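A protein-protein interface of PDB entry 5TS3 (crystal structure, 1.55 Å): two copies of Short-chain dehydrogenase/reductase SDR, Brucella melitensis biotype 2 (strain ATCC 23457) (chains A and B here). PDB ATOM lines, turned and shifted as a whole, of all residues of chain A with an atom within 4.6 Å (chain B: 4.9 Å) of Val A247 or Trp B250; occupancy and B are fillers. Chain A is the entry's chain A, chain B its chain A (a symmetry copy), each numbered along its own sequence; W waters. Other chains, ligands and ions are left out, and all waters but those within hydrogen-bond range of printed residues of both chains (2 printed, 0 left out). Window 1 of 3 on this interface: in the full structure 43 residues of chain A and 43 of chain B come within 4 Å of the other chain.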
ATOM      1  N   MET A 208     -30.898 -12.231  -9.105  1.00  0.00           N
ATOM      2  CA  MET A 208     -29.701 -12.927  -8.666  1.00  0.00           C
ATOM      3  C   MET A 208     -29.866 -14.399  -8.985  1.00  0.00           C
ATOM      4  O   MET A 208     -30.959 -14.945  -8.821  1.00  0.00           O
ATOM      5  CB  MET A 208     -29.494 -12.749  -7.158  1.00  0.00           C
ATOM      6  CG  MET A 208     -29.540 -11.306  -6.705  1.00  0.00           C
ATOM      7  SD  MET A 208     -29.302 -11.168  -4.932  1.00  0.00           S
ATOM      8  CE  MET A 208     -30.765 -12.010  -4.329  1.00  0.00           C
ATOM      9  N   GLU A 243     -23.148 -13.208   1.278  1.00  0.00           N
ATOM     10  CA  GLU A 243     -22.625 -12.777  -0.011  1.00  0.00           C
ATOM     11  C   GLU A 243     -23.748 -12.572  -1.015  1.00  0.00           C
ATOM     12  O   GLU A 243     -23.676 -11.671  -1.855  1.00  0.00           O
ATOM     13  CB  GLU A 243     -21.615 -13.800  -0.523  1.00  0.00           C
ATOM     14  CG  GLU A 243     -20.363 -13.852   0.347  1.00  0.00           C
ATOM     15  CD  GLU A 243     -19.360 -14.886  -0.147  1.00  0.00           C
ATOM     16  OE1 GLU A 243     -19.683 -16.097  -0.137  1.00  0.00           O
ATOM     17  OE2 GLU A 243     -18.268 -14.476  -0.576  1.00  0.00           O
ATOM     18  N   VAL A 244     -24.782 -13.411  -0.966  1.00  0.00           N
ATOM     19  CA  VAL A 244     -25.974 -13.132  -1.765  1.00  0.00           C
ATOM     20  C   VAL A 244     -26.628 -11.844  -1.287  1.00  0.00           C
ATOM     21  O   VAL A 244     -27.066 -11.013  -2.090  1.00  0.00           O
ATOM     22  CB  VAL A 244     -26.965 -14.310  -1.709  1.00  0.00           C
ATOM     23  CG1 VAL A 244     -28.228 -13.975  -2.538  1.00  0.00           C
ATOM     24  CG2 VAL A 244     -26.316 -15.609  -2.204  1.00  0.00           C
ATOM     25  N   ALA A 245     -26.699 -11.655   0.030  1.00  0.00           N
ATOM     26  CA  ALA A 245     -27.331 -10.449   0.560  1.00  0.00           C
ATOM     27  C   ALA A 245     -26.607  -9.186   0.100  1.00  0.00           C
ATOM     28  O   ALA A 245     -27.254  -8.161  -0.167  1.00  0.00           O
ATOM     29  CB  ALA A 245     -27.393 -10.524   2.087  1.00  0.00           C
ATOM     30  N   ASP A 246     -25.267  -9.241  -0.015  1.00  0.00           N
ATOM     31  CA  ASP A 246     -24.514  -8.078  -0.491  1.00  0.00           C
ATOM     32  C   ASP A 246     -24.936  -7.691  -1.903  1.00  0.00           C
ATOM     33  O   ASP A 246     -24.964  -6.502  -2.246  1.00  0.00           O
ATOM     34  CB  ASP A 246     -23.013  -8.365  -0.474  1.00  0.00           C
ATOM     35  CG  ASP A 246     -22.357  -8.041   0.848  1.00  0.00           C
ATOM     36  OD1 ASP A 246     -22.992  -7.377   1.703  1.00  0.00           O
ATOM     37  OD2 ASP A 246     -21.189  -8.457   1.016  1.00  0.00           O
ATOM     38  N   VAL A 247     -25.256  -8.681  -2.738  1.00  0.00           N
ATOM     39  CA  VAL A 247     -25.681  -8.392  -4.100  1.00  0.00           C
ATOM     40  C   VAL A 247     -27.062  -7.752  -4.091  1.00  0.00           C
ATOM     41  O   VAL A 247     -27.318  -6.791  -4.823  1.00  0.00           O
ATOM     42  CB  VAL A 247     -25.634  -9.680  -4.945  1.00  0.00           C
ATOM     43  CG1 VAL A 247     -26.104  -9.403  -6.369  1.00  0.00           C
ATOM     44  CG2 VAL A 247     -24.214 -10.227  -4.970  1.00  0.00           C
ATOM     45  N   ALA A 248     -27.964  -8.243  -3.235  1.00  0.00           N
ATOM     46  CA  ALA A 248     -29.292  -7.636  -3.148  1.00  0.00           C
ATOM     47  C   ALA A 248     -29.216  -6.200  -2.640  1.00  0.00           C
ATOM     48  O   ALA A 248     -29.945  -5.325  -3.126  1.00  0.00           O
ATOM     49  CB  ALA A 248     -30.195  -8.482  -2.247  1.00  0.00           C
ATOM     50  N   LEU A 249     -28.349  -5.939  -1.659  1.00  0.00           N
ATOM     51  CA  LEU A 249     -28.127  -4.564  -1.213  1.00  0.00           C
ATOM     52  C   LEU A 249     -27.682  -3.685  -2.371  1.00  0.00           C
ATOM     53  O   LEU A 249     -28.215  -2.588  -2.574  1.00  0.00           O
ATOM     54  CB  LEU A 249     -27.080  -4.528  -0.096  1.00  0.00           C
ATOM     55  CG  LEU A 249     -27.445  -5.076   1.284  1.00  0.00           C
ATOM     56  CD1 LEU A 249     -26.217  -5.024   2.198  1.00  0.00           C
ATOM     57  CD2 LEU A 249     -28.609  -4.276   1.878  1.00  0.00           C
ATOM     58  N   TRP A 250     -26.711  -4.159  -3.153  1.00  0.00           N
ATOM     59  CA  TRP A 250     -26.152  -3.320  -4.209  1.00  0.00           C
ATOM     60  C   TRP A 250     -27.170  -3.060  -5.308  1.00  0.00           C
ATOM     61  O   TRP A 250     -27.315  -1.915  -5.774  1.00  0.00           O
ATOM     62  CB  TRP A 250     -24.896  -3.966  -4.791  1.00  0.00           C
ATOM     63  CG  TRP A 250     -24.286  -3.116  -5.850  1.00  0.00           C
ATOM     64  CD1 TRP A 250     -23.633  -1.928  -5.678  1.00  0.00           C
ATOM     65  CD2 TRP A 250     -24.295  -3.374  -7.251  1.00  0.00           C
ATOM     66  NE1 TRP A 250     -23.223  -1.430  -6.900  1.00  0.00           N
ATOM     67  CE2 TRP A 250     -23.630  -2.294  -7.880  1.00  0.00           C
ATOM     68  CE3 TRP A 250     -24.800  -4.410  -8.038  1.00  0.00           C
ATOM     69  CZ2 TRP A 250     -23.443  -2.239  -9.258  1.00  0.00           C
ATOM     70  CZ3 TRP A 250     -24.617  -4.343  -9.425  1.00  0.00           C
ATOM     71  CH2 TRP A 250     -23.941  -3.268 -10.006  1.00  0.00           C
ATOM     72  N   LEU A 251     -27.916  -4.098  -5.704  1.00  0.00           N
ATOM     73  CA  LEU A 251     -28.905  -3.964  -6.768  1.00  0.00           C
ATOM     74  C   LEU A 251     -30.072  -3.064  -6.385  1.00  0.00           C
ATOM     75  O   LEU A 251     -30.827  -2.645  -7.269  1.00  0.00           O
ATOM     76  CB  LEU A 251     -29.439  -5.343  -7.165  1.00  0.00           C
ATOM     77  CG  LEU A 251     -28.468  -6.248  -7.909  1.00  0.00           C
ATOM     78  CD1 LEU A 251     -29.088  -7.639  -8.013  1.00  0.00           C
ATOM     79  CD2 LEU A 251     -28.158  -5.691  -9.310  1.00  0.00           C
ATOM     80  N   VAL A 266     -24.445 -15.538  -8.458  1.00  0.00           N
ATOM     81  CA  VAL A 266     -23.667 -15.431  -7.228  1.00  0.00           C
ATOM     82  C   VAL A 266     -23.205 -16.842  -6.877  1.00  0.00           C
ATOM     83  O   VAL A 266     -23.856 -17.546  -6.097  1.00  0.00           O
ATOM     84  CB  VAL A 266     -24.487 -14.779  -6.092  1.00  0.00           C
ATOM     85  CG1 VAL A 266     -23.559 -14.383  -4.946  1.00  0.00           C
ATOM     86  CG2 VAL A 266     -25.260 -13.534  -6.598  1.00  0.00           C
ATOM     87  N   ASP B 246     -19.432   3.173 -10.968  1.00  0.00           N
ATOM     88  CA  ASP B 246     -19.974   2.565  -9.750  1.00  0.00           C
ATOM     89  C   ASP B 246     -19.982   1.045  -9.851  1.00  0.00           C
ATOM     90  O   ASP B 246     -19.768   0.347  -8.852  1.00  0.00           O
ATOM     91  CB  ASP B 246     -21.396   3.061  -9.488  1.00  0.00           C
ATOM     92  CG  ASP B 246     -21.445   4.334  -8.676  1.00  0.00           C
ATOM     93  OD1 ASP B 246     -20.405   4.739  -8.104  1.00  0.00           O
ATOM     94  OD2 ASP B 246     -22.548   4.923  -8.614  1.00  0.00           O
ATOM     95  N   VAL B 247     -20.241   0.514 -11.048  1.00  0.00           N
ATOM     96  CA  VAL B 247     -20.255  -0.930 -11.229  1.00  0.00           C
ATOM     97  C   VAL B 247     -18.840  -1.484 -11.122  1.00  0.00           C
ATOM     98  O   VAL B 247     -18.614  -2.522 -10.495  1.00  0.00           O
ATOM     99  CB  VAL B 247     -20.924  -1.280 -12.573  1.00  0.00           C
ATOM    100  CG1 VAL B 247     -20.922  -2.790 -12.794  1.00  0.00           C
ATOM    101  CG2 VAL B 247     -22.355  -0.762 -12.585  1.00  0.00           C
ATOM    102  N   ALA B 248     -17.858  -0.781 -11.695  1.00  0.00           N
ATOM    103  CA  ALA B 248     -16.473  -1.238 -11.583  1.00  0.00           C
ATOM    104  C   ALA B 248     -15.994  -1.211 -10.136  1.00  0.00           C
ATOM    105  O   ALA B 248     -15.277  -2.121  -9.696  1.00  0.00           O
ATOM    106  CB  ALA B 248     -15.567  -0.383 -12.471  1.00  0.00           C
ATOM    107  N   LEU B 249     -16.367  -0.174  -9.383  1.00  0.00           N
ATOM    108  CA  LEU B 249     -16.057  -0.145  -7.954  1.00  0.00           C
ATOM    109  C   LEU B 249     -16.631  -1.365  -7.251  1.00  0.00           C
ATOM    110  O   LEU B 249     -15.936  -2.036  -6.479  1.00  0.00           O
ATOM    111  CB  LEU B 249     -16.604   1.134  -7.315  1.00  0.00           C
ATOM    112  CG  LEU B 249     -15.938   2.471  -7.639  1.00  0.00           C
ATOM    113  CD1 LEU B 249     -16.715   3.608  -6.966  1.00  0.00           C
ATOM    114  CD2 LEU B 249     -14.475   2.458  -7.183  1.00  0.00           C
ATOM    115  N   TRP B 250     -17.900  -1.676  -7.518  1.00  0.00           N
ATOM    116  CA  TRP B 250     -18.552  -2.760  -6.790  1.00  0.00           C
ATOM    117  C   TRP B 250     -17.948  -4.109  -7.145  1.00  0.00           C
ATOM    118  O   TRP B 250     -17.681  -4.935  -6.253  1.00  0.00           O
ATOM    119  CB  TRP B 250     -20.054  -2.760  -7.071  1.00  0.00           C
ATOM    120  CG  TRP B 250     -20.750  -3.838  -6.316  1.00  0.00           C
ATOM    121  CD1 TRP B 250     -20.971  -3.888  -4.968  1.00  0.00           C
ATOM    122  CD2 TRP B 250     -21.295  -5.036  -6.860  1.00  0.00           C
ATOM    123  NE1 TRP B 250     -21.635  -5.054  -4.639  1.00  0.00           N
ATOM    124  CE2 TRP B 250     -21.831  -5.780  -5.782  1.00  0.00           C
ATOM    125  CE3 TRP B 250     -21.380  -5.557  -8.152  1.00  0.00           C
ATOM    126  CZ2 TRP B 250     -22.464  -7.006  -5.968  1.00  0.00           C
ATOM    127  CZ3 TRP B 250     -22.008  -6.795  -8.330  1.00  0.00           C
ATOM    128  CH2 TRP B 250     -22.541  -7.491  -7.243  1.00  0.00           C
ATOM    129  N   LEU B 251     -17.682  -4.335  -8.437  1.00  0.00           N
ATOM    130  CA  LEU B 251     -17.124  -5.605  -8.890  1.00  0.00           C
ATOM    131  C   LEU B 251     -15.706  -5.843  -8.390  1.00  0.00           C
ATOM    132  O   LEU B 251     -15.223  -6.978  -8.462  1.00  0.00           O
ATOM    133  CB  LEU B 251     -17.138  -5.668 -10.420  1.00  0.00           C
ATOM    134  CG  LEU B 251     -18.506  -5.807 -11.072  1.00  0.00           C
ATOM    135  CD1 LEU B 251     -18.344  -5.623 -12.578  1.00  0.00           C
ATOM    136  CD2 LEU B 251     -19.126  -7.182 -10.762  1.00  0.00           C
ATOM    137  N   THR B 252     -15.019  -4.798  -7.930  1.00  0.00           N
ATOM    138  CA  THR B 252     -13.676  -4.933  -7.381  1.00  0.00           C
ATOM    139  C   THR B 252     -13.679  -4.808  -5.865  1.00  0.00           C
ATOM    140  O   THR B 252     -12.606  -4.724  -5.255  1.00  0.00           O
ATOM    141  CB  THR B 252     -12.740  -3.885  -7.984  1.00  0.00           C
ATOM    142  OG1 THR B 252     -13.246  -2.569  -7.716  1.00  0.00           O
ATOM    143  CG2 THR B 252     -12.599  -4.098  -9.502  1.00  0.00           C
ATOM    144  N   SER B 253     -14.856  -4.789  -5.248  1.00  0.00           N
ATOM    145  CA  SER B 253     -14.991  -4.574  -3.816  1.00  0.00           C
ATOM    146  C   SER B 253     -15.316  -5.880  -3.107  1.00  0.00           C
ATOM    147  O   SER B 253     -15.738  -6.861  -3.721  1.00  0.00           O
ATOM    148  CB  SER B 253     -16.093  -3.553  -3.515  1.00  0.00           C
ATOM    149  OG  SER B 253     -17.382  -4.160  -3.548  1.00  0.00           O
ATOM    150  N   GLU B 255     -17.831  -6.424  -1.459  1.00  0.00           N
ATOM    151  CA  GLU B 255     -19.275  -6.645  -1.444  1.00  0.00           C
ATOM    152  C   GLU B 255     -19.784  -7.359  -2.695  1.00  0.00           C
ATOM    153  O   GLU B 255     -21.003  -7.480  -2.879  1.00  0.00           O
ATOM    154  CB  GLU B 255     -20.013  -5.318  -1.220  1.00  0.00           C
ATOM    155  CG  GLU B 255     -19.750  -4.805   0.193  1.00  0.00           C
ATOM    156  CD  GLU B 255     -20.425  -3.493   0.502  1.00  0.00           C
ATOM    157  OE1 GLU B 255     -21.517  -3.243  -0.036  1.00  0.00           O
ATOM    158  OE2 GLU B 255     -19.855  -2.715   1.301  1.00  0.00           O
ATOM    159  N   SER B 256     -18.878  -7.859  -3.536  1.00  0.00           N
ATOM    160  CA  SER B 256     -19.216  -8.791  -4.602  1.00  0.00           C
ATOM    161  C   SER B 256     -18.384 -10.065  -4.483  1.00  0.00           C
ATOM    162  O   SER B 256     -18.070 -10.700  -5.488  1.00  0.00           O
ATOM    163  CB  SER B 256     -19.036  -8.137  -5.977  1.00  0.00           C
ATOM    164  OG  SER B 256     -17.694  -7.696  -6.191  1.00  0.00           O
ATOM    165  N   VAL B 259     -19.081 -13.164  -6.559  1.00  0.00           N
ATOM    166  CA  VAL B 259     -19.525 -12.892  -7.927  1.00  0.00           C
ATOM    167  C   VAL B 259     -18.323 -12.984  -8.863  1.00  0.00           C
ATOM    168  O   VAL B 259     -17.385 -12.183  -8.761  1.00  0.00           O
ATOM    169  CB  VAL B 259     -20.180 -11.508  -8.038  1.00  0.00           C
ATOM    170  CG1 VAL B 259     -20.598 -11.225  -9.492  1.00  0.00           C
ATOM    171  CG2 VAL B 259     -21.366 -11.390  -7.090  1.00  0.00           C
HETATM  172  O   HOH W   1     -23.416  -4.129  -1.663  1.00  0.00           O
HETATM  173  O   HOH W   2     -20.094 -10.169  -0.912  1.00  0.00           O
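Among the printed residues, merely in contact across the chains: Asp A246 with Glu B255 (3.3 Å), Trp A250 with Trp B250 (3.4 Å), Val A247 with Val B259 (3.7 Å), Val A247 with Trp B250 (3.8 Å) and Trp A250 with Val B247 (3.8 Å).
Water W1 lies within hydrogen-bond range of OE1 of Glu B255 (2.7 Å) and O of Asp A246 (2.9 Å).
Water W2 lies within hydrogen-bond range of the side-chain carboxylate (OD2) of Asp A246 (2.8 Å) and the backbone carbonyl oxygen (O) of Glu B255 (3.5 Å).
OG of Ser B253 is in hydrogen-bond range of O of Trp B250, 2.8 Å away.
O of Glu B255 is in hydrogen-bond range of NE1 of Trp B250, at 3.1 Å.
O of Trp B250 lies within hydrogen-bond range of OG of Ser B256 (2.8 Å).
The side-chain hydroxyl (OG) of Ser B253 sits close to the backbone NH (N) of Glu B255 (3.1 Å).
Along chain B the printed residues that touch a printed residue of chain A span positions 247 to 259.
Of the 11 printed residues of chain A, 3 touch a printed residue of chain B.
Hydrophobic or aromatic side chains of chain A within 4 Å of the printed part of chain B: Val A247 and Trp A250.
Of chain A, only Val A247 (3.8 Å) and Trp A250 (3.4 Å) come within 4 Å of Trp B250.
Of the printed residues of chain A, Glu B255 touches Asp A246 (3.3 Å).
Printed residues of chain B within 4 Å of Trp A250: Val B247 (3.8 Å) and Trp B250 (3.4 Å).
Of the printed residues of chain B, Asp A246 touches Glu B255.
Printed residues of chain A within 4 Å of Val B259: Val A247.
Of the printed residues of chain A, Val B247 touches Trp A250.
The nearest residue of chain B that does not touch Val A247 is Glu B255 (4.4 Å).
Val A247 touches Trp B250, and with the chains exchanged Trp A250 touches Val B247.
Trp A250 touches its own counterpart, Trp B250.
Positions printed for both chains: 246, 247, 248, 249, 250 and 251.
Of the 5 pairs that touch across the chains among the printed residues, 3 have their exchanged pair printed and touching as well.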
